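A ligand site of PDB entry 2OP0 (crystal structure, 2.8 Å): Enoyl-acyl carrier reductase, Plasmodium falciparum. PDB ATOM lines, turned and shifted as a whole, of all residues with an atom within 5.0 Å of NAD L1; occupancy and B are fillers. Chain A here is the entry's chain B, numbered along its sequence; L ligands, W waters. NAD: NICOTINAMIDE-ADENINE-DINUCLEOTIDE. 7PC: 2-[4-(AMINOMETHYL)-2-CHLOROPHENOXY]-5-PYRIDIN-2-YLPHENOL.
Water W2 lies within hydrogen-bond range of O2B of NAD L1, N of Trp 44 and O of Ile 18. Water W4 lies within hydrogen-bond range of an oxygen (O3D) of NAD L1 (2.9 Å), the backbone NH of Leu 178 (3.1 Å) and the backbone NH of Leu 129 (3.5 Å). Water W3 lies within hydrogen-bond range of the side-chain carboxylate (OD1) of Asp 20, the backbone NH (N) of Arg 231 and an oxygen (O2A) of NAD L1. Water W1 lies within hydrogen-bond range of N of Gly 25 (2.9 Å), O of Gly 17 (3.0 Å) and O2A of NAD L1 (3.2 Å).
The side-chain hydroxyl (OG) of Ser 230 is in hydrogen-bond range of the backbone NH (N) of Ala 233 (3.3 Å). The side-chain amino group of Lys 198 is in hydrogen-bond range of the backbone carbonyl oxygen of Leu 178 (3.0 Å). OH of Tyr 24 sits at hydrogen-bond distance from O of Gly 226 (2.7 Å). The side-chain carboxylate of Asp 81 lies within hydrogen-bond range of the indole nitrogen of Trp 44 (3.5 Å). OG of Ser 83 sits at hydrogen-bond distance from OD1 of Asp 81 (2.5 Å). O of Thr 179 is in hydrogen-bond range of N of Ala 225, 3.1 Å away. O of Phe 80 lies close to N of Trp 44 (3.5 Å).
An oxygen (O2N) of NAD L1 lies within hydrogen-bond range of the side-chain hydroxyl (OG) of Ser 230 (2.6 Å). The side-chain amino group (NZ) of Lys 198 sits at hydrogen-bond distance from an oxygen (O2D) of NAD L1 (2.8 Å). The backbone NH (N) of Tyr 24 sits at hydrogen-bond distance from an oxygen (O1N) of NAD L1 (2.8 Å). An oxygen (O7N) of NAD L1 lies within hydrogen-bond range of the backbone NH (N) of Leu 228 (2.9 Å). N7N of NAD L1 lies within hydrogen-bond range of O of Leu 228 (3.0 Å). The backbone NH (N) of Ala 82 sits at hydrogen-bond distance from a nitrogen (N1A) of NAD L1 (2.9 Å). A nitrogen (N7A) of NAD L1 lies within hydrogen-bond range of the side-chain amide nitrogen (ND2) of Asn 131, 3.0 Å away. The backbone NH (N) of Gly 19 sits at hydrogen-bond distance from an oxygen (O3B) of NAD L1. The side-chain carboxylate (OD1) of Asp 81 sits at hydrogen-bond distance from a nitrogen (N6A) of NAD L1 (3.1 Å). N of Ala 232 sits close to O1A of NAD L1, at 3.3 Å. O3D of NAD L1 sits at hydrogen-bond distance from O of Leu 129. The side-chain amide oxygen (OD1) of Asn 131 is in hydrogen-bond range of a nitrogen (N30) of 7PC L2 (3.3 Å). An oxygen (O22) of 7PC L2 lies within hydrogen-bond range of the side-chain hydroxyl of Tyr 190, 2.5 Å away.
NE1 of Trp 44 sits close to N6A of NAD L1 (3.4 Å). The backbone carbonyl oxygen (O) of Gly 226 lies close to an oxygen (O7N) of NAD L1, at 3.5 Å. Merely in contact with NAD L1: Leu 178, Pro 227, Ser 128, Thr 179, Gly 23, Ala 225, Phe 80, Ala 130, Ile 282, Tyr 180, Gly 17, Arg 231, Ser 83, Ala 233 and Ile 18. Hydrophobic or aromatic side chains that line NAD L1: Tyr 24, Trp 44, Phe 80, Ala 82, Leu 129, Ala 130, Leu 178, Tyr 180, Ala 225, Leu 228, Ala 232, Ala 233 and Ile 282. 27 residues have an atom within 4 Å of NAD L1: Gly 17, Ile 18, Gly 19, Gly 23, Tyr 24, Trp 44, Phe 80, Asp 81, Ala 82, Ser 83, Ser 128, Leu 129, Ala 130, Asn 131, Leu 178, Thr 179, Tyr 180, Lys 198, Ala 225, Gly 226, Pro 227, Leu 228, Ser 230, Arg 231, Ala 232, Ala 233 and Ile 282. Along chain A the residues within 4 Å of NAD L1 span positions 17 to 282. The nearest printed residue that does not touch NAD L1 is Val 47 (4.2 Å).
An oxygen (O2D) of NAD L1 sits at hydrogen-bond distance from an oxygen (O22) of 7PC L2.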
ATOM      1  N   GLY A  17      -9.929   7.271  22.955  1.00  0.00           N
ATOM      2  CA  GLY A  17     -11.089   7.931  23.526  1.00  0.00           C
ATOM      3  C   GLY A  17     -10.750   8.964  24.581  1.00  0.00           C
ATOM      4  O   GLY A  17     -11.017   8.767  25.779  1.00  0.00           O
ATOM      5  N   ILE A  18     -10.157  10.070  24.153  1.00  0.00           N
ATOM      6  CA  ILE A  18      -9.973  11.212  25.033  1.00  0.00           C
ATOM      7  C   ILE A  18     -10.356  12.444  24.240  1.00  0.00           C
ATOM      8  O   ILE A  18      -9.780  12.715  23.194  1.00  0.00           O
ATOM      9  CB  ILE A  18      -8.536  11.316  25.573  1.00  0.00           C
ATOM     10  CG1 ILE A  18      -8.323  12.662  26.250  1.00  0.00           C
ATOM     11  CG2 ILE A  18      -7.520  11.125  24.461  1.00  0.00           C
ATOM     12  CD1 ILE A  18      -6.883  12.929  26.633  1.00  0.00           C
ATOM     13  N   GLY A  19     -11.345  13.173  24.731  1.00  0.00           N
ATOM     14  CA  GLY A  19     -11.847  14.345  24.033  1.00  0.00           C
ATOM     15  C   GLY A  19     -11.391  15.624  24.691  1.00  0.00           C
ATOM     16  O   GLY A  19     -11.422  16.687  24.088  1.00  0.00           O
ATOM     17  N   ASP A  20     -10.987  15.520  25.959  1.00  0.00           N
ATOM     18  CA  ASP A  20     -10.481  16.674  26.685  1.00  0.00           C
ATOM     19  C   ASP A  20      -9.706  16.238  27.907  1.00  0.00           C
ATOM     20  O   ASP A  20      -9.179  15.130  27.959  1.00  0.00           O
ATOM     21  CB  ASP A  20     -11.622  17.627  27.079  1.00  0.00           C
ATOM     22  CG  ASP A  20     -12.702  16.939  27.888  1.00  0.00           C
ATOM     23  OD1 ASP A  20     -12.360  16.162  28.807  1.00  0.00           O
ATOM     24  OD2 ASP A  20     -13.896  17.167  27.602  1.00  0.00           O
ATOM     25  N   ASN A  22     -10.891  16.414  31.113  1.00  0.00           N
ATOM     26  CA  ASN A  22     -11.789  16.187  32.240  1.00  0.00           C
ATOM     27  C   ASN A  22     -12.241  14.740  32.377  1.00  0.00           C
ATOM     28  O   ASN A  22     -13.076  14.418  33.222  1.00  0.00           O
ATOM     29  CB  ASN A  22     -12.986  17.120  32.113  1.00  0.00           C
ATOM     30  CG  ASN A  22     -12.579  18.530  31.775  1.00  0.00           C
ATOM     31  OD1 ASN A  22     -11.958  19.219  32.584  1.00  0.00           O
ATOM     32  ND2 ASN A  22     -12.904  18.970  30.561  1.00  0.00           N
ATOM     33  N   GLY A  23     -11.691  13.865  31.544  1.00  0.00           N
ATOM     34  CA  GLY A  23     -12.119  12.491  31.511  1.00  0.00           C
ATOM     35  C   GLY A  23     -11.161  11.546  32.208  1.00  0.00           C
ATOM     36  O   GLY A  23     -10.190  11.980  32.835  1.00  0.00           O
ATOM     37  N   TYR A  24     -11.460  10.247  32.083  1.00  0.00           N
ATOM     38  CA  TYR A  24     -10.611   9.217  32.651  1.00  0.00           C
ATOM     39  C   TYR A  24      -9.434   8.977  31.740  1.00  0.00           C
ATOM     40  O   TYR A  24      -8.357   8.626  32.206  1.00  0.00           O
ATOM     41  CB  TYR A  24     -11.381   7.915  32.865  1.00  0.00           C
ATOM     42  CG  TYR A  24     -12.205   7.935  34.123  1.00  0.00           C
ATOM     43  CD1 TYR A  24     -11.602   8.166  35.357  1.00  0.00           C
ATOM     44  CD2 TYR A  24     -13.582   7.744  34.089  1.00  0.00           C
ATOM     45  CE1 TYR A  24     -12.332   8.203  36.510  1.00  0.00           C
ATOM     46  CE2 TYR A  24     -14.320   7.771  35.248  1.00  0.00           C
ATOM     47  CZ  TYR A  24     -13.691   8.006  36.456  1.00  0.00           C
ATOM     48  OH  TYR A  24     -14.416   8.035  37.635  1.00  0.00           O
ATOM     49  N   GLY A  25      -9.639   9.161  30.452  1.00  0.00           N
ATOM     50  CA  GLY A  25      -8.540   9.068  29.509  1.00  0.00           C
ATOM     51  C   GLY A  25      -7.383   9.996  29.848  1.00  0.00           C
ATOM     52  O   GLY A  25      -6.212   9.584  29.801  1.00  0.00           O
ATOM     53  N   TRP A  44     -11.761  11.287  18.625  1.00  0.00           N
ATOM     54  CA  TRP A  44     -12.959  11.340  17.800  1.00  0.00           C
ATOM     55  C   TRP A  44     -12.965  12.622  16.977  1.00  0.00           C
ATOM     56  O   TRP A  44     -12.783  13.709  17.526  1.00  0.00           O
ATOM     57  CB  TRP A  44     -14.156  11.324  18.726  1.00  0.00           C
ATOM     58  CG  TRP A  44     -15.436  10.787  18.173  1.00  0.00           C
ATOM     59  CD1 TRP A  44     -15.592   9.805  17.235  1.00  0.00           C
ATOM     60  CD2 TRP A  44     -16.765  11.169  18.569  1.00  0.00           C
ATOM     61  NE1 TRP A  44     -16.920   9.568  17.008  1.00  0.00           N
ATOM     62  CE2 TRP A  44     -17.668  10.377  17.820  1.00  0.00           C
ATOM     63  CE3 TRP A  44     -17.269  12.093  19.485  1.00  0.00           C
ATOM     64  CZ2 TRP A  44     -19.056  10.491  17.962  1.00  0.00           C
ATOM     65  CZ3 TRP A  44     -18.657  12.207  19.627  1.00  0.00           C
ATOM     66  CH2 TRP A  44     -19.529  11.407  18.869  1.00  0.00           C
ATOM     67  N   VAL A  47     -14.451  16.240  17.596  1.00  0.00           N
ATOM     68  CA  VAL A  47     -13.815  17.092  18.603  1.00  0.00           C
ATOM     69  C   VAL A  47     -12.309  17.215  18.404  1.00  0.00           C
ATOM     70  O   VAL A  47     -11.615  17.787  19.242  1.00  0.00           O
ATOM     71  CB  VAL A  47     -14.014  16.545  20.033  1.00  0.00           C
ATOM     72  CG1 VAL A  47     -15.495  16.235  20.276  1.00  0.00           C
ATOM     73  CG2 VAL A  47     -13.136  15.313  20.252  1.00  0.00           C
ATOM     74  N   PHE A  80      -9.545   9.279  15.294  1.00  0.00           N
ATOM     75  CA  PHE A  80      -9.894   7.898  15.569  1.00  0.00           C
ATOM     76  C   PHE A  80     -11.393   7.753  15.790  1.00  0.00           C
ATOM     77  O   PHE A  80     -11.967   8.452  16.620  1.00  0.00           O
ATOM     78  CB  PHE A  80      -9.137   7.391  16.794  1.00  0.00           C
ATOM     79  CG  PHE A  80      -9.604   6.062  17.286  1.00  0.00           C
ATOM     80  CD1 PHE A  80      -9.368   4.921  16.541  1.00  0.00           C
ATOM     81  CD2 PHE A  80     -10.273   5.945  18.488  1.00  0.00           C
ATOM     82  CE1 PHE A  80      -9.796   3.695  16.993  1.00  0.00           C
ATOM     83  CE2 PHE A  80     -10.700   4.723  18.948  1.00  0.00           C
ATOM     84  CZ  PHE A  80     -10.475   3.589  18.200  1.00  0.00           C
ATOM     85  N   ASP A  81     -12.014   6.854  15.037  1.00  0.00           N
ATOM     86  CA  ASP A  81     -13.438   6.614  15.187  1.00  0.00           C
ATOM     87  C   ASP A  81     -13.745   5.146  15.378  1.00  0.00           C
ATOM     88  O   ASP A  81     -13.654   4.355  14.440  1.00  0.00           O
ATOM     89  CB  ASP A  81     -14.224   7.173  14.017  1.00  0.00           C
ATOM     90  CG  ASP A  81     -15.694   7.324  14.325  1.00  0.00           C
ATOM     91  OD1 ASP A  81     -16.141   6.663  15.295  1.00  0.00           O
ATOM     92  OD2 ASP A  81     -16.398   8.099  13.647  1.00  0.00           O
ATOM     93  N   ALA A  82     -14.140   4.794  16.595  1.00  0.00           N
ATOM     94  CA  ALA A  82     -14.271   3.405  17.013  1.00  0.00           C
ATOM     95  C   ALA A  82     -15.505   2.698  16.460  1.00  0.00           C
ATOM     96  O   ALA A  82     -15.780   1.548  16.785  1.00  0.00           O
ATOM     97  CB  ALA A  82     -14.232   3.320  18.522  1.00  0.00           C
ATOM     98  N   SER A  83     -16.234   3.392  15.600  1.00  0.00           N
ATOM     99  CA  SER A  83     -17.412   2.795  14.989  1.00  0.00           C
ATOM    100  C   SER A  83     -17.063   2.236  13.629  1.00  0.00           C
ATOM    101  O   SER A  83     -17.885   1.562  12.995  1.00  0.00           O
ATOM    102  CB  SER A  83     -18.535   3.820  14.902  1.00  0.00           C
ATOM    103  OG  SER A  83     -18.033   5.110  14.670  1.00  0.00           O
ATOM    104  N   SER A 128     -11.232   3.672  26.267  1.00  0.00           N
ATOM    105  CA  SER A 128     -11.791   4.637  27.201  1.00  0.00           C
ATOM    106  C   SER A 128     -12.911   5.447  26.582  1.00  0.00           C
ATOM    107  O   SER A 128     -12.999   6.659  26.757  1.00  0.00           O
ATOM    108  CB  SER A 128     -10.701   5.572  27.709  1.00  0.00           C
ATOM    109  OG  SER A 128     -11.247   6.351  28.744  1.00  0.00           O
ATOM    110  N   LEU A 129     -13.767   4.762  25.844  1.00  0.00           N
ATOM    111  CA  LEU A 129     -14.787   5.446  25.078  1.00  0.00           C
ATOM    112  C   LEU A 129     -16.093   4.703  25.229  1.00  0.00           C
ATOM    113  O   LEU A 129     -16.108   3.496  25.449  1.00  0.00           O
ATOM    114  CB  LEU A 129     -14.368   5.516  23.607  1.00  0.00           C
ATOM    115  CG  LEU A 129     -14.301   4.167  22.887  1.00  0.00           C
ATOM    116  CD1 LEU A 129     -15.620   3.914  22.165  1.00  0.00           C
ATOM    117  CD2 LEU A 129     -13.134   4.113  21.897  1.00  0.00           C
ATOM    118  N   ALA A 130     -17.195   5.442  25.122  1.00  0.00           N
ATOM    119  CA  ALA A 130     -18.526   4.887  25.228  1.00  0.00           C
ATOM    120  C   ALA A 130     -19.466   5.848  24.533  1.00  0.00           C
ATOM    121  O   ALA A 130     -19.167   7.041  24.409  1.00  0.00           O
ATOM    122  CB  ALA A 130     -18.905   4.741  26.688  1.00  0.00           C
ATOM    123  N   ASN A 131     -20.596   5.353  24.069  1.00  0.00           N
ATOM    124  CA  ASN A 131     -21.557   6.228  23.417  1.00  0.00           C
ATOM    125  C   ASN A 131     -22.876   5.531  23.190  1.00  0.00           C
ATOM    126  O   ASN A 131     -22.906   4.316  22.970  1.00  0.00           O
ATOM    127  CB  ASN A 131     -20.996   6.727  22.095  1.00  0.00           C
ATOM    128  CG  ASN A 131     -21.264   8.190  21.883  1.00  0.00           C
ATOM    129  OD1 ASN A 131     -22.240   8.739  22.417  1.00  0.00           O
ATOM    130  ND2 ASN A 131     -20.398   8.849  21.117  1.00  0.00           N
ATOM    131  N   LYS A 153     -20.727   0.852  19.870  1.00  0.00           N
ATOM    132  CA  LYS A 153     -19.679   1.829  20.150  1.00  0.00           C
ATOM    133  C   LYS A 153     -19.025   1.656  21.510  1.00  0.00           C
ATOM    134  O   LYS A 153     -17.933   2.147  21.721  1.00  0.00           O
ATOM    135  CB  LYS A 153     -20.222   3.241  19.962  1.00  0.00           C
ATOM    136  CG  LYS A 153     -21.135   3.326  18.755  1.00  0.00           C
ATOM    137  CD  LYS A 153     -21.021   4.640  18.017  1.00  0.00           C
ATOM    138  CE  LYS A 153     -21.687   4.541  16.635  1.00  0.00           C
ATOM    139  NZ  LYS A 153     -22.464   5.779  16.283  1.00  0.00           N
ATOM    140  N   LEU A 178     -12.927   0.660  30.494  1.00  0.00           N
ATOM    141  CA  LEU A 178     -13.607   1.243  31.656  1.00  0.00           C
ATOM    142  C   LEU A 178     -15.068   0.839  31.665  1.00  0.00           C
ATOM    143  O   LEU A 178     -15.722   0.799  30.621  1.00  0.00           O
ATOM    144  CB  LEU A 178     -13.488   2.769  31.630  1.00  0.00           C
ATOM    145  CG  LEU A 178     -12.262   3.384  32.305  1.00  0.00           C
ATOM    146  CD1 LEU A 178     -11.007   2.978  31.603  1.00  0.00           C
ATOM    147  CD2 LEU A 178     -12.381   4.869  32.284  1.00  0.00           C
ATOM    148  N   THR A 179     -15.589   0.541  32.843  1.00  0.00           N
ATOM    149  CA  THR A 179     -16.979   0.108  32.950  1.00  0.00           C
ATOM    150  C   THR A 179     -17.671   0.788  34.133  1.00  0.00           C
ATOM    151  O   THR A 179     -17.046   1.534  34.892  1.00  0.00           O
ATOM    152  CB  THR A 179     -17.075  -1.438  33.040  1.00  0.00           C
ATOM    153  OG1 THR A 179     -18.442  -1.842  33.198  1.00  0.00           O
ATOM    154  CG2 THR A 179     -16.254  -1.978  34.186  1.00  0.00           C
ATOM    155  N   TYR A 180     -18.975   0.562  34.277  1.00  0.00           N
ATOM    156  CA  TYR A 180     -19.710   1.120  35.389  1.00  0.00           C
ATOM    157  C   TYR A 180     -20.649   0.083  36.033  1.00  0.00           C
ATOM    158  O   TYR A 180     -21.215  -0.769  35.355  1.00  0.00           O
ATOM    159  CB  TYR A 180     -20.464   2.387  34.943  1.00  0.00           C
ATOM    160  CG  TYR A 180     -21.223   3.078  36.037  1.00  0.00           C
ATOM    161  CD1 TYR A 180     -20.583   3.557  37.159  1.00  0.00           C
ATOM    162  CD2 TYR A 180     -22.596   3.264  35.942  1.00  0.00           C
ATOM    163  CE1 TYR A 180     -21.276   4.193  38.152  1.00  0.00           C
ATOM    164  CE2 TYR A 180     -23.299   3.899  36.936  1.00  0.00           C
ATOM    165  CZ  TYR A 180     -22.640   4.358  38.032  1.00  0.00           C
ATOM    166  OH  TYR A 180     -23.353   4.991  39.028  1.00  0.00           O
ATOM    167  N   TYR A 190     -29.321   5.538  33.931  1.00  0.00           N
ATOM    168  CA  TYR A 190     -28.187   5.190  33.098  1.00  0.00           C
ATOM    169  C   TYR A 190     -28.733   4.383  31.928  1.00  0.00           C
ATOM    170  O   TYR A 190     -28.648   3.156  31.916  1.00  0.00           O
ATOM    171  CB  TYR A 190     -27.188   4.374  33.930  1.00  0.00           C
ATOM    172  CG  TYR A 190     -25.854   4.113  33.285  1.00  0.00           C
ATOM    173  CD1 TYR A 190     -24.868   5.103  33.239  1.00  0.00           C
ATOM    174  CD2 TYR A 190     -25.545   2.858  32.768  1.00  0.00           C
ATOM    175  CE1 TYR A 190     -23.634   4.834  32.673  1.00  0.00           C
ATOM    176  CE2 TYR A 190     -24.322   2.601  32.207  1.00  0.00           C
ATOM    177  CZ  TYR A 190     -23.376   3.581  32.159  1.00  0.00           C
ATOM    178  OH  TYR A 190     -22.178   3.279  31.588  1.00  0.00           O
ATOM    179  N   LYS A 198     -22.162  -2.108  29.202  1.00  0.00           N
ATOM    180  CA  LYS A 198     -21.238  -2.382  30.289  1.00  0.00           C
ATOM    181  C   LYS A 198     -21.335  -3.848  30.720  1.00  0.00           C
ATOM    182  O   LYS A 198     -20.327  -4.496  30.968  1.00  0.00           O
ATOM    183  CB  LYS A 198     -21.506  -1.458  31.476  1.00  0.00           C
ATOM    184  CG  LYS A 198     -21.178  -0.020  31.187  1.00  0.00           C
ATOM    185  CD  LYS A 198     -19.847   0.123  30.467  1.00  0.00           C
ATOM    186  CE  LYS A 198     -19.498   1.592  30.283  1.00  0.00           C
ATOM    187  NZ  LYS A 198     -18.257   1.851  29.492  1.00  0.00           N
ATOM    188  N   ALA A 225     -15.209   2.193  37.338  1.00  0.00           N
ATOM    189  CA  ALA A 225     -14.899   3.460  37.969  1.00  0.00           C
ATOM    190  C   ALA A 225     -16.118   4.081  38.653  1.00  0.00           C
ATOM    191  O   ALA A 225     -17.257   3.767  38.315  1.00  0.00           O
ATOM    192  CB  ALA A 225     -14.343   4.411  36.939  1.00  0.00           C
ATOM    193  N   GLY A 226     -15.863   4.969  39.606  1.00  0.00           N
ATOM    194  CA  GLY A 226     -16.929   5.736  40.241  1.00  0.00           C
ATOM    195  C   GLY A 226     -17.295   6.910  39.364  1.00  0.00           C
ATOM    196  O   GLY A 226     -16.835   6.990  38.230  1.00  0.00           O
ATOM    197  N   PRO A 227     -18.124   7.821  39.877  1.00  0.00           N
ATOM    198  CA  PRO A 227     -18.581   9.017  39.163  1.00  0.00           C
ATOM    199  C   PRO A 227     -17.517  10.112  39.061  1.00  0.00           C
ATOM    200  O   PRO A 227     -16.905  10.513  40.056  1.00  0.00           O
ATOM    201  CB  PRO A 227     -19.734   9.525  40.032  1.00  0.00           C
ATOM    202  CG  PRO A 227     -20.002   8.465  41.025  1.00  0.00           C
ATOM    203  CD  PRO A 227     -18.727   7.750  41.218  1.00  0.00           C
ATOM    204  N   LEU A 228     -17.317  10.585  37.835  1.00  0.00           N
ATOM    205  CA  LEU A 228     -16.425  11.690  37.551  1.00  0.00           C
ATOM    206  C   LEU A 228     -17.218  12.621  36.648  1.00  0.00           C
ATOM    207  O   LEU A 228     -17.974  12.162  35.792  1.00  0.00           O
ATOM    208  CB  LEU A 228     -15.189  11.173  36.815  1.00  0.00           C
ATOM    209  CG  LEU A 228     -14.005  12.119  36.676  1.00  0.00           C
ATOM    210  CD1 LEU A 228     -13.218  12.131  37.957  1.00  0.00           C
ATOM    211  CD2 LEU A 228     -13.132  11.686  35.525  1.00  0.00           C
ATOM    212  N   SER A 230     -17.164  14.041  33.879  1.00  0.00           N
ATOM    213  CA  SER A 230     -16.671  14.078  32.519  1.00  0.00           C
ATOM    214  C   SER A 230     -17.709  14.692  31.565  1.00  0.00           C
ATOM    215  O   SER A 230     -18.868  14.875  31.934  1.00  0.00           O
ATOM    216  CB  SER A 230     -16.319  12.665  32.053  1.00  0.00           C
ATOM    217  OG  SER A 230     -17.413  11.790  32.251  1.00  0.00           O
ATOM    218  N   ARG A 231     -17.256  15.008  30.362  1.00  0.00           N
ATOM    219  CA  ARG A 231     -18.129  15.511  29.305  1.00  0.00           C
ATOM    220  C   ARG A 231     -19.292  14.556  29.101  1.00  0.00           C
ATOM    221  O   ARG A 231     -20.457  14.947  29.102  1.00  0.00           O
ATOM    222  CB  ARG A 231     -17.321  15.629  28.014  1.00  0.00           C
ATOM    223  CG  ARG A 231     -18.039  16.289  26.857  1.00  0.00           C
ATOM    224  CD  ARG A 231     -17.235  16.103  25.569  1.00  0.00           C
ATOM    225  NE  ARG A 231     -17.632  17.043  24.519  1.00  0.00           N
ATOM    226  CZ  ARG A 231     -18.613  16.827  23.641  1.00  0.00           C
ATOM    227  NH1 ARG A 231     -19.315  15.703  23.674  1.00  0.00           N
ATOM    228  NH2 ARG A 231     -18.884  17.746  22.725  1.00  0.00           N
ATOM    229  N   ALA A 232     -18.956  13.285  28.946  1.00  0.00           N
ATOM    230  CA  ALA A 232     -19.932  12.233  28.664  1.00  0.00           C
ATOM    231  C   ALA A 232     -20.892  11.974  29.823  1.00  0.00           C
ATOM    232  O   ALA A 232     -22.026  11.549  29.606  1.00  0.00           O
ATOM    233  CB  ALA A 232     -19.210  10.955  28.282  1.00  0.00           C
ATOM    234  N   ALA A 233     -20.446  12.222  31.051  1.00  0.00           N
ATOM    235  CA  ALA A 233     -21.305  12.045  32.217  1.00  0.00           C
ATOM    236  C   ALA A 233     -22.511  12.992  32.174  1.00  0.00           C
ATOM    237  O   ALA A 233     -23.580  12.664  32.684  1.00  0.00           O
ATOM    238  CB  ALA A 233     -20.497  12.255  33.502  1.00  0.00           C
ATOM    239  N   ILE A 282     -25.120  12.658  38.079  1.00  0.00           N
ATOM    240  CA  ILE A 282     -23.664  12.726  38.100  1.00  0.00           C
ATOM    241  C   ILE A 282     -23.275  13.651  39.236  1.00  0.00           C
ATOM    242  O   ILE A 282     -22.476  13.293  40.084  1.00  0.00           O
ATOM    243  CB  ILE A 282     -23.015  13.192  36.786  1.00  0.00           C
ATOM    244  CG1 ILE A 282     -21.513  12.879  36.789  1.00  0.00           C
ATOM    245  CG2 ILE A 282     -23.242  14.681  36.537  1.00  0.00           C
ATOM    246  CD1 ILE A 282     -21.175  11.417  36.994  1.00  0.00           C
HETATM  247  PA  NAD L   1     -15.242  11.295  28.277  1.00  0.00           P
HETATM  248  O1A NAD L   1     -16.262  12.036  27.438  1.00  0.00           O
HETATM  249  O2A NAD L   1     -13.977  12.006  28.702  1.00  0.00           O
HETATM  250  O5B NAD L   1     -14.799   9.965  27.485  1.00  0.00           O
HETATM  251  C5B NAD L   1     -15.427   9.531  26.285  1.00  0.00           C
HETATM  252  C4B NAD L   1     -14.611  10.045  25.113  1.00  0.00           C
HETATM  253  O4B NAD L   1     -14.632   9.119  24.038  1.00  0.00           O
HETATM  254  C3B NAD L   1     -15.198  11.348  24.592  1.00  0.00           C
HETATM  255  O3B NAD L   1     -14.280  12.429  24.797  1.00  0.00           O
HETATM  256  C2B NAD L   1     -15.490  11.121  23.119  1.00  0.00           C
HETATM  257  O2B NAD L   1     -14.970  12.169  22.291  1.00  0.00           O
HETATM  258  C1B NAD L   1     -14.835   9.795  22.788  1.00  0.00           C
HETATM  259  N9A NAD L   1     -15.696   8.991  21.897  1.00  0.00           N
HETATM  260  C8A NAD L   1     -17.038   8.798  21.962  1.00  0.00           C
HETATM  261  N7A NAD L   1     -17.511   7.997  20.939  1.00  0.00           N
HETATM  262  C5A NAD L   1     -16.445   7.654  20.198  1.00  0.00           C
HETATM  263  C6A NAD L   1     -16.125   6.850  19.004  1.00  0.00           C
HETATM  264  N6A NAD L   1     -17.086   6.382  18.202  1.00  0.00           N
HETATM  265  N1A NAD L   1     -14.814   6.627  18.787  1.00  0.00           N
HETATM  266  C2A NAD L   1     -13.885   7.320  19.337  1.00  0.00           C
HETATM  267  N3A NAD L   1     -14.062   8.143  20.288  1.00  0.00           N
HETATM  268  C4A NAD L   1     -15.305   8.304  20.819  1.00  0.00           C
HETATM  269  O3  NAD L   1     -16.021  10.742  29.587  1.00  0.00           O
HETATM  270  PN  NAD L   1     -15.438   9.601  30.576  1.00  0.00           P
HETATM  271  O1N NAD L   1     -13.975   9.884  30.860  1.00  0.00           O
HETATM  272  O2N NAD L   1     -16.421   9.479  31.726  1.00  0.00           O
HETATM  273  O5D NAD L   1     -15.563   8.265  29.686  1.00  0.00           O
HETATM  274  C5D NAD L   1     -14.483   7.337  29.519  1.00  0.00           C
HETATM  275  C4D NAD L   1     -14.939   5.953  29.960  1.00  0.00           C
HETATM  276  O4D NAD L   1     -15.165   5.900  31.374  1.00  0.00           O
HETATM  277  C3D NAD L   1     -16.238   5.497  29.301  1.00  0.00           C
HETATM  278  O3D NAD L   1     -16.085   4.155  28.816  1.00  0.00           O
HETATM  279  C2D NAD L   1     -17.276   5.508  30.424  1.00  0.00           C
HETATM  280  O2D NAD L   1     -18.284   4.522  30.202  1.00  0.00           O
HETATM  281  C1D NAD L   1     -16.401   5.214  31.636  1.00  0.00           C
HETATM  282  N1N NAD L   1     -16.968   5.593  32.934  1.00  0.00           N
HETATM  283  C2N NAD L   1     -17.210   6.882  33.251  1.00  0.00           C
HETATM  284  C3N NAD L   1     -17.733   7.205  34.506  1.00  0.00           C
HETATM  285  C7N NAD L   1     -18.017   8.631  34.893  1.00  0.00           C
HETATM  286  O7N NAD L   1     -18.701   8.862  36.005  1.00  0.00           O
HETATM  287  N7N NAD L   1     -17.632   9.614  34.185  1.00  0.00           N
HETATM  288  C4N NAD L   1     -17.991   6.203  35.426  1.00  0.00           C
HETATM  289  C5N NAD L   1     -17.728   4.882  35.078  1.00  0.00           C
HETATM  290  C6N NAD L   1     -17.201   4.604  33.823  1.00  0.00           C
HETATM  291 CL2  7PC L   2     -18.464   8.225  28.136  1.00  0.00          CL
HETATM  292  C15 7PC L   2     -20.251   7.997  28.197  1.00  0.00           C
HETATM  293  C16 7PC L   2     -21.054   8.451  27.146  1.00  0.00           C
HETATM  294  C14 7PC L   2     -20.838   7.370  29.283  1.00  0.00           C
HETATM  295  C19 7PC L   2     -22.225   7.193  29.332  1.00  0.00           C
HETATM  296  C22 7PC L   2     -23.019   7.648  28.280  1.00  0.00           C
HETATM  297  C17 7PC L   2     -22.434   8.284  27.190  1.00  0.00           C
HETATM  298  C29 7PC L   2     -23.133   8.720  26.196  1.00  0.00           C
HETATM  299  N30 7PC L   2     -23.752   9.115  25.294  1.00  0.00           N
HETATM  300  O13 7PC L   2     -20.031   6.923  30.296  1.00  0.00           O
HETATM  301  C2  7PC L   2     -20.406   7.118  31.590  1.00  0.00           C
HETATM  302  C1  7PC L   2     -20.477   6.037  32.444  1.00  0.00           C
HETATM  303  O22 7PC L   2     -20.172   4.798  31.987  1.00  0.00           O
HETATM  304  C6  7PC L   2     -20.868   6.229  33.764  1.00  0.00           C
HETATM  305  C5  7PC L   2     -21.161   7.511  34.211  1.00  0.00           C
HETATM  306  C4  7PC L   2     -21.090   8.592  33.356  1.00  0.00           C
HETATM  307  C3  7PC L   2     -20.709   8.398  32.039  1.00  0.00           C
HETATM  308  C7  7PC L   2     -21.592   7.713  35.618  1.00  0.00           C
HETATM  309  N23 7PC L   2     -20.793   7.323  36.637  1.00  0.00           N
HETATM  310  C24 7PC L   2     -21.168   7.496  37.908  1.00  0.00           C
HETATM  311  C25 7PC L   2     -22.401   8.090  38.206  1.00  0.00           C
HETATM  312  C26 7PC L   2     -23.245   8.500  37.180  1.00  0.00           C
HETATM  313  C27 7PC L   2     -22.832   8.307  35.871  1.00  0.00           C
HETATM  314  O   HOH W   1     -11.667   9.824  28.492  1.00  0.00           O
HETATM  315  O   HOH W   2     -12.252  11.583  21.607  1.00  0.00           O
HETATM  316  O   HOH W   3     -14.645  14.947  29.576  1.00  0.00           O
HETATM  317  O   HOH W   4     -14.150   2.124  28.049  1.00  0.00           O
